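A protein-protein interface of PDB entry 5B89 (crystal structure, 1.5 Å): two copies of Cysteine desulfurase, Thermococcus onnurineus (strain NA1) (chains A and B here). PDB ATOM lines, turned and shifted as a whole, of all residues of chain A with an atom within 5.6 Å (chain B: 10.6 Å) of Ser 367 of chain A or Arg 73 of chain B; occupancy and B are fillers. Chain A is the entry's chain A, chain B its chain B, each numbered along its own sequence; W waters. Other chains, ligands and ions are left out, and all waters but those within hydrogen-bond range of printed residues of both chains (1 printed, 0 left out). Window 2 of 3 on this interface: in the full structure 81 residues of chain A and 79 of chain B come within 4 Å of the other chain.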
ATOM      1  N   GLU A  36     -22.879  15.849 -21.187  1.00  0.00           N
ATOM      2  CA  GLU A  36     -22.465  14.945 -20.136  1.00  0.00           C
ATOM      3  C   GLU A  36     -21.859  13.644 -20.546  1.00  0.00           C
ATOM      4  O   GLU A  36     -21.005  13.174 -19.887  1.00  0.00           O
ATOM      5  CB  GLU A  36     -23.638  14.577 -19.241  1.00  0.00           C
ATOM      6  CG  GLU A  36     -24.492  15.701 -18.794  1.00  0.00           C
ATOM      7  CD  GLU A  36     -23.740  16.737 -18.002  1.00  0.00           C
ATOM      8  OE1 GLU A  36     -24.098  17.906 -18.069  1.00  0.00           O
ATOM      9  OE2 GLU A  36     -22.788  16.387 -17.306  1.00  0.00           O
ATOM     10  N   VAL A  37     -22.350  13.067 -21.615  1.00  0.00           N
ATOM     11  CA  VAL A  37     -21.870  11.806 -22.100  1.00  0.00           C
ATOM     12  C   VAL A  37     -21.714  11.796 -23.603  1.00  0.00           C
ATOM     13  O   VAL A  37     -22.238  12.628 -24.254  1.00  0.00           O
ATOM     14  CB  VAL A  37     -22.854  10.676 -21.752  1.00  0.00           C
ATOM     15  CG1 VAL A  37     -23.011  10.570 -20.270  1.00  0.00           C
ATOM     16  CG2 VAL A  37     -24.189  10.942 -22.389  1.00  0.00           C
ATOM     17  N   ILE A  38     -20.981  10.815 -24.085  1.00  0.00           N
ATOM     18  CA  ILE A  38     -20.842  10.517 -25.465  1.00  0.00           C
ATOM     19  C   ILE A  38     -21.795   9.329 -25.594  1.00  0.00           C
ATOM     20  O   ILE A  38     -21.478   8.260 -25.182  1.00  0.00           O
ATOM     21  CB  ILE A  38     -19.415  10.097 -25.843  1.00  0.00           C
ATOM     22  CG1 ILE A  38     -18.489  11.313 -25.724  1.00  0.00           C
ATOM     23  CG2 ILE A  38     -19.394   9.536 -27.231  1.00  0.00           C
ATOM     24  CD1 ILE A  38     -17.030  11.044 -26.004  1.00  0.00           C
ATOM     25  N   TYR A  39     -22.980   9.575 -26.125  1.00  0.00           N
ATOM     26  CA  TYR A  39     -23.968   8.546 -26.209  1.00  0.00           C
ATOM     27  C   TYR A  39     -23.946   7.789 -27.507  1.00  0.00           C
ATOM     28  O   TYR A  39     -24.394   8.276 -28.466  1.00  0.00           O
ATOM     29  CB  TYR A  39     -25.349   9.166 -26.002  1.00  0.00           C
ATOM     30  CG  TYR A  39     -26.461   8.176 -25.885  1.00  0.00           C
ATOM     31  CD1 TYR A  39     -26.715   7.579 -24.702  1.00  0.00           C
ATOM     32  CD2 TYR A  39     -27.258   7.877 -26.953  1.00  0.00           C
ATOM     33  CE1 TYR A  39     -27.705   6.675 -24.587  1.00  0.00           C
ATOM     34  CE2 TYR A  39     -28.243   6.960 -26.850  1.00  0.00           C
ATOM     35  CZ  TYR A  39     -28.497   6.400 -25.641  1.00  0.00           C
ATOM     36  OH  TYR A  39     -29.483   5.518 -25.540  1.00  0.00           O
ATOM     37  N   LEU A 363     -15.376   1.851 -21.153  1.00  0.00           N
ATOM     38  CA  LEU A 363     -15.853   2.987 -21.910  1.00  0.00           C
ATOM     39  C   LEU A 363     -16.780   3.853 -21.032  1.00  0.00           C
ATOM     40  O   LEU A 363     -16.734   5.011 -21.086  1.00  0.00           O
ATOM     41  CB  LEU A 363     -16.563   2.532 -23.187  1.00  0.00           C
ATOM     42  CG  LEU A 363     -15.672   2.033 -24.329  1.00  0.00           C
ATOM     43  CD1 LEU A 363     -16.376   1.202 -25.377  1.00  0.00           C
ATOM     44  CD2 LEU A 363     -14.921   3.175 -24.957  1.00  0.00           C
ATOM     45  N   ASP A 364     -17.615   3.230 -20.206  1.00  0.00           N
ATOM     46  CA  ASP A 364     -18.512   3.960 -19.343  1.00  0.00           C
ATOM     47  C   ASP A 364     -17.726   4.833 -18.393  1.00  0.00           C
ATOM     48  O   ASP A 364     -18.080   5.918 -18.130  1.00  0.00           O
ATOM     49  CB  ASP A 364     -19.448   2.985 -18.631  1.00  0.00           C
ATOM     50  CG  ASP A 364     -20.426   3.666 -17.709  1.00  0.00           C
ATOM     51  OD1 ASP A 364     -21.254   4.407 -18.112  1.00  0.00           O
ATOM     52  OD2 ASP A 364     -20.291   3.466 -16.539  1.00  0.00           O
ATOM     53  N   ASP A 365     -16.619   4.319 -17.902  1.00  0.00           N
ATOM     54  CA  ASP A 365     -15.741   5.173 -17.106  1.00  0.00           C
ATOM     55  C   ASP A 365     -15.264   6.443 -17.771  1.00  0.00           C
ATOM     56  O   ASP A 365     -15.098   7.468 -17.135  1.00  0.00           O
ATOM     57  CB  ASP A 365     -14.502   4.378 -16.741  1.00  0.00           C
ATOM     58  CG  ASP A 365     -14.711   3.554 -15.547  1.00  0.00           C
ATOM     59  OD1 ASP A 365     -15.897   3.464 -15.030  1.00  0.00           O
ATOM     60  OD2 ASP A 365     -13.694   2.965 -15.120  1.00  0.00           O
ATOM     61  N   HIS A 366     -15.163   6.389 -19.089  1.00  0.00           N
ATOM     62  CA  HIS A 366     -14.798   7.569 -19.850  1.00  0.00           C
ATOM     63  C   HIS A 366     -16.006   8.343 -20.358  1.00  0.00           C
ATOM     64  O   HIS A 366     -15.922   9.225 -21.237  1.00  0.00           O
ATOM     65  CB  HIS A 366     -13.911   7.122 -20.979  1.00  0.00           C
ATOM     66  CG  HIS A 366     -12.548   6.690 -20.532  1.00  0.00           C
ATOM     67  ND1 HIS A 366     -12.245   5.402 -20.151  1.00  0.00           N
ATOM     68  CD2 HIS A 366     -11.406   7.389 -20.415  1.00  0.00           C
ATOM     69  CE1 HIS A 366     -10.971   5.315 -19.815  1.00  0.00           C
ATOM     70  NE2 HIS A 366     -10.448   6.503 -19.986  1.00  0.00           N
ATOM     71  N   SER A 367     -17.198   8.064 -19.803  1.00  0.00           N
ATOM     72  CA  SER A 367     -18.440   8.728 -20.192  1.00  0.00           C
ATOM     73  C   SER A 367     -18.848   8.394 -21.599  1.00  0.00           C
ATOM     74  O   SER A 367     -19.599   9.200 -22.171  1.00  0.00           O
ATOM     75  CB  SER A 367     -18.522  10.216 -19.851  1.00  0.00           C
ATOM     76  OG  SER A 367     -18.270  10.496 -18.447  1.00  0.00           O
ATOM     77  N   ILE A 368     -18.467   7.242 -22.103  1.00  0.00           N
ATOM     78  CA  ILE A 368     -18.900   6.789 -23.374  1.00  0.00           C
ATOM     79  C   ILE A 368     -19.896   5.627 -23.152  1.00  0.00           C
ATOM     80  O   ILE A 368     -19.546   4.575 -22.588  1.00  0.00           O
ATOM     81  CB  ILE A 368     -17.705   6.359 -24.263  1.00  0.00           C
ATOM     82  CG1 ILE A 368     -16.695   7.533 -24.448  1.00  0.00           C
ATOM     83  CG2 ILE A 368     -18.189   5.804 -25.535  1.00  0.00           C
ATOM     84  CD1 ILE A 368     -15.402   7.006 -25.018  1.00  0.00           C
ATOM     85  N   MET A 369     -21.127   5.808 -23.652  1.00  0.00           N
ATOM     86  CA  MET A 369     -22.174   4.790 -23.454  1.00  0.00           C
ATOM     87  C   MET A 369     -22.332   3.861 -24.631  1.00  0.00           C
ATOM     88  O   MET A 369     -22.666   4.356 -25.757  1.00  0.00           O
ATOM     89  CB  MET A 369     -23.497   5.490 -23.197  1.00  0.00           C
ATOM     90  CG  MET A 369     -23.514   6.669 -22.306  1.00  0.00           C
ATOM     91  SD  MET A 369     -23.384   6.289 -20.569  1.00  0.00           S
ATOM     92  CE  MET A 369     -21.654   6.717 -20.138  1.00  0.00           C
ATOM     93  N   TYR B  59     -36.562  11.943 -16.603  1.00  0.00           N
ATOM     94  CA  TYR B  59     -36.116  10.780 -17.327  1.00  0.00           C
ATOM     95  C   TYR B  59     -35.653  11.193 -18.745  1.00  0.00           C
ATOM     96  O   TYR B  59     -34.624  10.835 -19.171  1.00  0.00           O
ATOM     97  CB  TYR B  59     -37.237   9.710 -17.479  1.00  0.00           C
ATOM     98  CG  TYR B  59     -36.937   8.625 -18.523  1.00  0.00           C
ATOM     99  CD1 TYR B  59     -35.929   7.759 -18.356  1.00  0.00           C
ATOM    100  CD2 TYR B  59     -37.665   8.520 -19.678  1.00  0.00           C
ATOM    101  CE1 TYR B  59     -35.632   6.812 -19.278  1.00  0.00           C
ATOM    102  CE2 TYR B  59     -37.389   7.560 -20.618  1.00  0.00           C
ATOM    103  CZ  TYR B  59     -36.381   6.699 -20.419  1.00  0.00           C
ATOM    104  OH  TYR B  59     -36.078   5.765 -21.337  1.00  0.00           O
ATOM    105  N   LYS B  62     -32.508  13.906 -18.340  1.00  0.00           N
ATOM    106  CA  LYS B  62     -31.386  13.616 -17.477  1.00  0.00           C
ATOM    107  C   LYS B  62     -30.879  12.195 -17.364  1.00  0.00           C
ATOM    108  O   LYS B  62     -29.756  12.009 -17.035  1.00  0.00           O
ATOM    109  CB  LYS B  62     -31.603  14.201 -16.065  1.00  0.00           C
ATOM    110  CG  LYS B  62     -31.824  15.700 -16.020  1.00  0.00           C
ATOM    111  CD  LYS B  62     -31.747  16.198 -14.581  1.00  0.00           C
ATOM    112  CE  LYS B  62     -32.379  17.553 -14.367  1.00  0.00           C
ATOM    113  NZ  LYS B  62     -32.396  18.334 -15.616  1.00  0.00           N
ATOM    114  N   TYR B  63     -31.705  11.199 -17.633  1.00  0.00           N
ATOM    115  CA  TYR B  63     -31.248   9.823 -17.563  1.00  0.00           C
ATOM    116  C   TYR B  63     -31.852   8.917 -18.627  1.00  0.00           C
ATOM    117  O   TYR B  63     -32.156   7.835 -18.394  1.00  0.00           O
ATOM    118  CB  TYR B  63     -31.363   9.201 -16.143  1.00  0.00           C
ATOM    119  CG  TYR B  63     -32.736   9.113 -15.506  1.00  0.00           C
ATOM    120  CD1 TYR B  63     -33.245  10.146 -14.831  1.00  0.00           C
ATOM    121  CD2 TYR B  63     -33.441   7.945 -15.529  1.00  0.00           C
ATOM    122  CE1 TYR B  63     -34.483  10.087 -14.239  1.00  0.00           C
ATOM    123  CE2 TYR B  63     -34.677   7.869 -14.952  1.00  0.00           C
ATOM    124  CZ  TYR B  63     -35.196   8.946 -14.306  1.00  0.00           C
ATOM    125  OH  TYR B  63     -36.405   8.888 -13.732  1.00  0.00           O
ATOM    126  N   ARG B  64     -31.973   9.460 -19.813  1.00  0.00           N
ATOM    127  CA  ARG B  64     -32.583   8.783 -20.909  1.00  0.00           C
ATOM    128  C   ARG B  64     -31.806   7.591 -21.409  1.00  0.00           C
ATOM    129  O   ARG B  64     -30.703   7.723 -21.885  1.00  0.00           O
ATOM    130  CB  ARG B  64     -32.823   9.819 -22.030  1.00  0.00           C
ATOM    131  CG  ARG B  64     -33.584   9.300 -23.226  1.00  0.00           C
ATOM    132  CD  ARG B  64     -35.045   8.957 -22.998  1.00  0.00           C
ATOM    133  NE  ARG B  64     -35.601   8.761 -24.315  1.00  0.00           N
ATOM    134  CZ  ARG B  64     -35.755   7.625 -24.947  1.00  0.00           C
ATOM    135  NH1 ARG B  64     -36.075   7.656 -26.215  1.00  0.00           N
ATOM    136  NH2 ARG B  64     -35.621   6.481 -24.342  1.00  0.00           N
ATOM    137  N   ALA B  65     -32.428   6.428 -21.330  1.00  0.00           N
ATOM    138  CA  ALA B  65     -31.835   5.223 -21.799  1.00  0.00           C
ATOM    139  C   ALA B  65     -32.838   4.112 -21.744  1.00  0.00           C
ATOM    140  O   ALA B  65     -33.818   4.285 -21.176  1.00  0.00           O
ATOM    141  CB  ALA B  65     -30.636   4.860 -20.922  1.00  0.00           C
ATOM    142  N   ASN B  66     -32.483   2.998 -22.348  1.00  0.00           N
ATOM    143  CA  ASN B  66     -33.265   1.800 -22.330  1.00  0.00           C
ATOM    144  C   ASN B  66     -32.904   1.033 -21.035  1.00  0.00           C
ATOM    145  O   ASN B  66     -31.942   1.320 -20.420  1.00  0.00           O
ATOM    146  CB  ASN B  66     -33.105   0.946 -23.592  1.00  0.00           C
ATOM    147  CG  ASN B  66     -34.387   0.230 -23.958  1.00  0.00           C
ATOM    148  OD1 ASN B  66     -35.105  -0.207 -23.088  1.00  0.00           O
ATOM    149  ND2 ASN B  66     -34.626   0.064 -25.212  1.00  0.00           N
ATOM    150  N   VAL B  67     -33.726   0.072 -20.664  1.00  0.00           N
ATOM    151  CA  VAL B  67     -33.512  -0.642 -19.434  1.00  0.00           C
ATOM    152  C   VAL B  67     -32.813  -1.950 -19.631  1.00  0.00           C
ATOM    153  O   VAL B  67     -31.911  -2.027 -20.393  1.00  0.00           O
ATOM    154  CB  VAL B  67     -34.833  -0.781 -18.671  1.00  0.00           C
ATOM    155  CG1 VAL B  67     -35.295   0.574 -18.243  1.00  0.00           C
ATOM    156  CG2 VAL B  67     -35.938  -1.394 -19.515  1.00  0.00           C
ATOM    157  N   ARG B  69     -30.736  -3.596 -17.684  1.00  0.00           N
ATOM    158  CA  ARG B  69     -29.405  -3.562 -17.127  1.00  0.00           C
ATOM    159  C   ARG B  69     -28.240  -3.500 -18.099  1.00  0.00           C
ATOM    160  O   ARG B  69     -27.297  -4.259 -17.982  1.00  0.00           O
ATOM    161  CB  ARG B  69     -29.217  -4.728 -16.142  1.00  0.00           C
ATOM    162  CG  ARG B  69     -29.979  -4.543 -14.837  1.00  0.00           C
ATOM    163  CD  ARG B  69     -29.568  -3.303 -14.008  1.00  0.00           C
ATOM    164  NE  ARG B  69     -30.297  -3.253 -12.733  1.00  0.00           N
ATOM    165  CZ  ARG B  69     -30.373  -2.198 -11.932  1.00  0.00           C
ATOM    166  NH1 ARG B  69     -29.769  -1.066 -12.279  1.00  0.00           N
ATOM    167  NH2 ARG B  69     -31.109  -2.260 -10.811  1.00  0.00           N
ATOM    168  N   GLY B  70     -28.319  -2.584 -19.036  1.00  0.00           N
ATOM    169  CA  GLY B  70     -27.222  -2.351 -19.944  1.00  0.00           C
ATOM    170  C   GLY B  70     -26.083  -1.898 -19.051  1.00  0.00           C
ATOM    171  O   GLY B  70     -26.285  -1.321 -18.024  1.00  0.00           O
ATOM    172  N   VAL B  71     -24.883  -2.168 -19.472  1.00  0.00           N
ATOM    173  CA  VAL B  71     -23.752  -1.857 -18.664  1.00  0.00           C
ATOM    174  C   VAL B  71     -23.615  -0.408 -18.280  1.00  0.00           C
ATOM    175  O   VAL B  71     -23.245  -0.165 -17.207  1.00  0.00           O
ATOM    176  CB  VAL B  71     -22.467  -2.466 -19.260  1.00  0.00           C
ATOM    177  CG1 VAL B  71     -21.216  -2.038 -18.512  1.00  0.00           C
ATOM    178  CG2 VAL B  71     -22.609  -3.980 -19.230  1.00  0.00           C
ATOM    179  N   HIS B  72     -23.945   0.528 -19.139  1.00  0.00           N
ATOM    180  CA  HIS B  72     -23.687   1.917 -18.905  1.00  0.00           C
ATOM    181  C   HIS B  72     -24.493   2.631 -17.891  1.00  0.00           C
ATOM    182  O   HIS B  72     -25.552   2.215 -17.596  1.00  0.00           O
ATOM    183  CB  HIS B  72     -23.590   2.702 -20.239  1.00  0.00           C
ATOM    184  CG  HIS B  72     -24.846   2.728 -21.048  1.00  0.00           C
ATOM    185  ND1 HIS B  72     -25.918   3.519 -20.725  1.00  0.00           N
ATOM    186  CD2 HIS B  72     -25.176   2.102 -22.186  1.00  0.00           C
ATOM    187  CE1 HIS B  72     -26.848   3.382 -21.636  1.00  0.00           C
ATOM    188  NE2 HIS B  72     -26.429   2.523 -22.534  1.00  0.00           N
ATOM    189  N   ARG B  73     -23.974   3.718 -17.390  1.00  0.00           N
ATOM    190  CA  ARG B  73     -24.615   4.431 -16.321  1.00  0.00           C
ATOM    191  C   ARG B  73     -25.980   4.930 -16.569  1.00  0.00           C
ATOM    192  O   ARG B  73     -26.740   4.949 -15.664  1.00  0.00           O
ATOM    193  CB  ARG B  73     -23.772   5.549 -15.736  1.00  0.00           C
ATOM    194  CG  ARG B  73     -23.629   6.809 -16.542  1.00  0.00           C
ATOM    195  CD  ARG B  73     -22.874   7.794 -15.643  1.00  0.00           C
ATOM    196  NE  ARG B  73     -22.525   9.059 -16.234  1.00  0.00           N
ATOM    197  CZ  ARG B  73     -21.305   9.391 -16.665  1.00  0.00           C
ATOM    198  NH1 ARG B  73     -20.292   8.565 -16.546  1.00  0.00           N
ATOM    199  NH2 ARG B  73     -21.119  10.579 -17.180  1.00  0.00           N
ATOM    200  N   LEU B  74     -26.266   5.352 -17.791  1.00  0.00           N
ATOM    201  CA  LEU B  74     -27.666   5.863 -18.039  1.00  0.00           C
ATOM    202  C   LEU B  74     -28.613   4.671 -18.036  1.00  0.00           C
ATOM    203  O   LEU B  74     -29.696   4.818 -17.458  1.00  0.00           O
ATOM    204  CB  LEU B  74     -27.720   6.556 -19.428  1.00  0.00           C
ATOM    205  CG  LEU B  74     -26.954   7.862 -19.483  1.00  0.00           C
ATOM    206  CD1 LEU B  74     -27.084   8.437 -20.878  1.00  0.00           C
ATOM    207  CD2 LEU B  74     -27.304   8.931 -18.545  1.00  0.00           C
ATOM    208  N   SER B  75     -28.294   3.507 -18.551  1.00  0.00           N
ATOM    209  CA  SER B  75     -29.121   2.341 -18.543  1.00  0.00           C
ATOM    210  C   SER B  75     -29.283   1.913 -17.090  1.00  0.00           C
ATOM    211  O   SER B  75     -30.333   1.457 -16.696  1.00  0.00           O
ATOM    212  CB  SER B  75     -28.651   1.227 -19.392  1.00  0.00           C
ATOM    213  OG  SER B  75     -29.548   0.093 -19.414  1.00  0.00           O
ATOM    214  N   GLN B  76     -28.208   2.013 -16.334  1.00  0.00           N
ATOM    215  CA  GLN B  76     -28.379   1.556 -14.904  1.00  0.00           C
ATOM    216  C   GLN B  76     -29.343   2.414 -14.208  1.00  0.00           C
ATOM    217  O   GLN B  76     -30.231   1.851 -13.438  1.00  0.00           O
ATOM    218  CB  GLN B  76     -26.998   1.556 -14.210  1.00  0.00           C
ATOM    219  CG  GLN B  76     -26.063   0.434 -14.656  1.00  0.00           C
ATOM    220  CD  GLN B  76     -26.493  -0.993 -14.304  1.00  0.00           C
ATOM    221  OE1 GLN B  76     -26.909  -1.213 -13.158  1.00  0.00           O
ATOM    222  NE2 GLN B  76     -26.336  -1.953 -15.173  1.00  0.00           N
ATOM    223  N   MET B  77     -29.323   3.716 -14.416  1.00  0.00           N
ATOM    224  CA  MET B  77     -30.175   4.678 -13.723  1.00  0.00           C
ATOM    225  C   MET B  77     -31.626   4.424 -14.217  1.00  0.00           C
ATOM    226  O   MET B  77     -32.594   4.328 -13.415  1.00  0.00           O
ATOM    227  CB  MET B  77     -29.845   6.170 -13.918  1.00  0.00           C
ATOM    228  CG  MET B  77     -30.753   7.082 -13.170  1.00  0.00           C
ATOM    229  SD  MET B  77     -30.904   6.788 -11.357  1.00  0.00           S
ATOM    230  CE  MET B  77     -29.256   7.194 -10.757  1.00  0.00           C
ATOM    231  N   ALA B  78     -31.813   4.344 -15.515  1.00  0.00           N
ATOM    232  CA  ALA B  78     -33.161   4.024 -16.068  1.00  0.00           C
ATOM    233  C   ALA B  78     -33.733   2.721 -15.543  1.00  0.00           C
ATOM    234  O   ALA B  78     -34.892   2.708 -15.176  1.00  0.00           O
ATOM    235  CB  ALA B  78     -33.143   4.067 -17.614  1.00  0.00           C
ATOM    236  N   THR B  79     -32.942   1.683 -15.512  1.00  0.00           N
ATOM    237  CA  THR B  79     -33.355   0.374 -15.016  1.00  0.00           C
ATOM    238  C   THR B  79     -33.731   0.524 -13.520  1.00  0.00           C
ATOM    239  O   THR B  79     -34.804  -0.001 -13.118  1.00  0.00           O
ATOM    240  CB  THR B  79     -32.272  -0.683 -15.180  1.00  0.00           C
ATOM    241  OG1 THR B  79     -31.992  -0.822 -16.557  1.00  0.00           O
ATOM    242  CG2 THR B  79     -32.759  -1.981 -14.676  1.00  0.00           C
ATOM    243  N   HIS B  80     -32.909   1.180 -12.719  1.00  0.00           N
ATOM    244  CA  HIS B  80     -33.277   1.366 -11.278  1.00  0.00           C
ATOM    245  C   HIS B  80     -34.557   2.085 -11.148  1.00  0.00           C
ATOM    246  O   HIS B  80     -35.422   1.635 -10.347  1.00  0.00           O
ATOM    247  CB  HIS B  80     -32.170   2.137 -10.592  1.00  0.00           C
ATOM    248  CG  HIS B  80     -32.522   2.820  -9.280  1.00  0.00           C
ATOM    249  ND1 HIS B  80     -32.602   2.108  -8.097  1.00  0.00           N
ATOM    250  CD2 HIS B  80     -32.837   4.102  -8.969  1.00  0.00           C
ATOM    251  CE1 HIS B  80     -32.966   2.924  -7.123  1.00  0.00           C
ATOM    252  NE2 HIS B  80     -33.105   4.142  -7.621  1.00  0.00           N
ATOM    253  N   LYS B  81     -34.811   3.185 -11.883  1.00  0.00           N
ATOM    254  CA  LYS B  81     -36.044   3.953 -11.753  1.00  0.00           C
ATOM    255  C   LYS B  81     -37.238   3.126 -12.304  1.00  0.00           C
ATOM    256  O   LYS B  81     -38.377   3.250 -11.755  1.00  0.00           O
ATOM    257  CB  LYS B  81     -35.941   5.320 -12.442  1.00  0.00           C
ATOM    258  CG  LYS B  81     -34.983   6.230 -11.702  1.00  0.00           C
ATOM    259  CD  LYS B  81     -35.451   6.699 -10.379  1.00  0.00           C
ATOM    260  CE  LYS B  81     -36.549   7.622 -10.458  1.00  0.00           C
ATOM    261  NZ  LYS B  81     -37.024   8.176  -9.142  1.00  0.00           N
HETATM  262  O   HOH W   1     -29.780   3.189 -23.787  1.00  0.00           O
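N of Ile 38 of chain A is in hydrogen-bond range of O of Ser 367 of chain A, at 2.9 Å.
The backbone carbonyl oxygen (O) of Ile 38 of chain A sits at hydrogen-bond distance from the backbone NH (N) of Met 369 of chain A (2.9 Å).
The backbone NH (N) of Leu 74 of chain B lies close to a ring nitrogen (ND1) of His 72 of chain B, at 3.5 Å.
The backbone NH (N) of Ser 75 of chain B is in hydrogen-bond range of a ring nitrogen (ND1) of His 72 of chain B (3.2 Å).
N of Arg 73 of chain B lies within hydrogen-bond range of OD1 of Asp 364 of chain A (2.9 Å).
The side-chain hydroxyl of Ser 367 of chain A lies within hydrogen-bond range of the guanidinium group of Arg 73 of chain B, at 3.1 Å.
The side-chain sulfur (SD) of Met 369 of chain A sits close to a ring nitrogen (ND1) of His 72 of chain B (3.8 Å).
Arg 73 of chain B touches Glu 36 of chain A.
Arg 73 of chain B touches Val 37 of chain A (NH2 to CG1, 3.6 Å).
CD1 of Leu 74 of chain B touches CD1 of Tyr 39 of chain A, at 3.9 Å.
OD1 of Asp 364 of chain A touches CA of His 72 of chain B, at 3.6 Å.
Hydrophobic or aromatic side chains of chain A that line the printed part of chain B: Val 37, Tyr 39 and Met 369.
Among the printed residues, no Asp or Glu carboxylate lies within 4 Å of a Lys or Arg side-chain nitrogen of the other chain.
Water W1 lies within hydrogen-bond range of OH of Tyr 39 of chain A (2.9 Å) and N of Asn 66 of chain B (3.1 Å).
No position is printed for both chains.
Printed residues of chain B within 4 Å of Glu 36 of chain A: Arg 73 (3.8 Å).
Of the printed residues of chain B, Val 37 of chain A touches Arg 73 (3.6 Å).
Printed residues of chain B within 4 Å of Tyr 39 of chain A: Leu 74.
His 366 of chain A touches none of the printed residues of chain B.
No residue of chain B comes within 4 Å of Ile 368 of chain A.
Of the printed residues of chain A, His 72 of chain B touches Asp 364 (3.6 Å) and Met 369 (3.6 Å).
Of chain A, only Glu 36, Val 37, Asp 364 and Ser 367 come within 4 Å of Arg 73 of chain B.
Printed residues of chain A within 4 Å of Leu 74 of chain B: Tyr 39 (3.9 Å).
Ser 75 of chain B touches none of the printed residues of chain A.
The nearest residue of chain B that does not touch Ser 367 of chain A is His 72 of chain B (7.5 Å).
The nearest printed residue of chain A that does not touch Leu 74 of chain B is Met 369 of chain A (4.05 Å).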
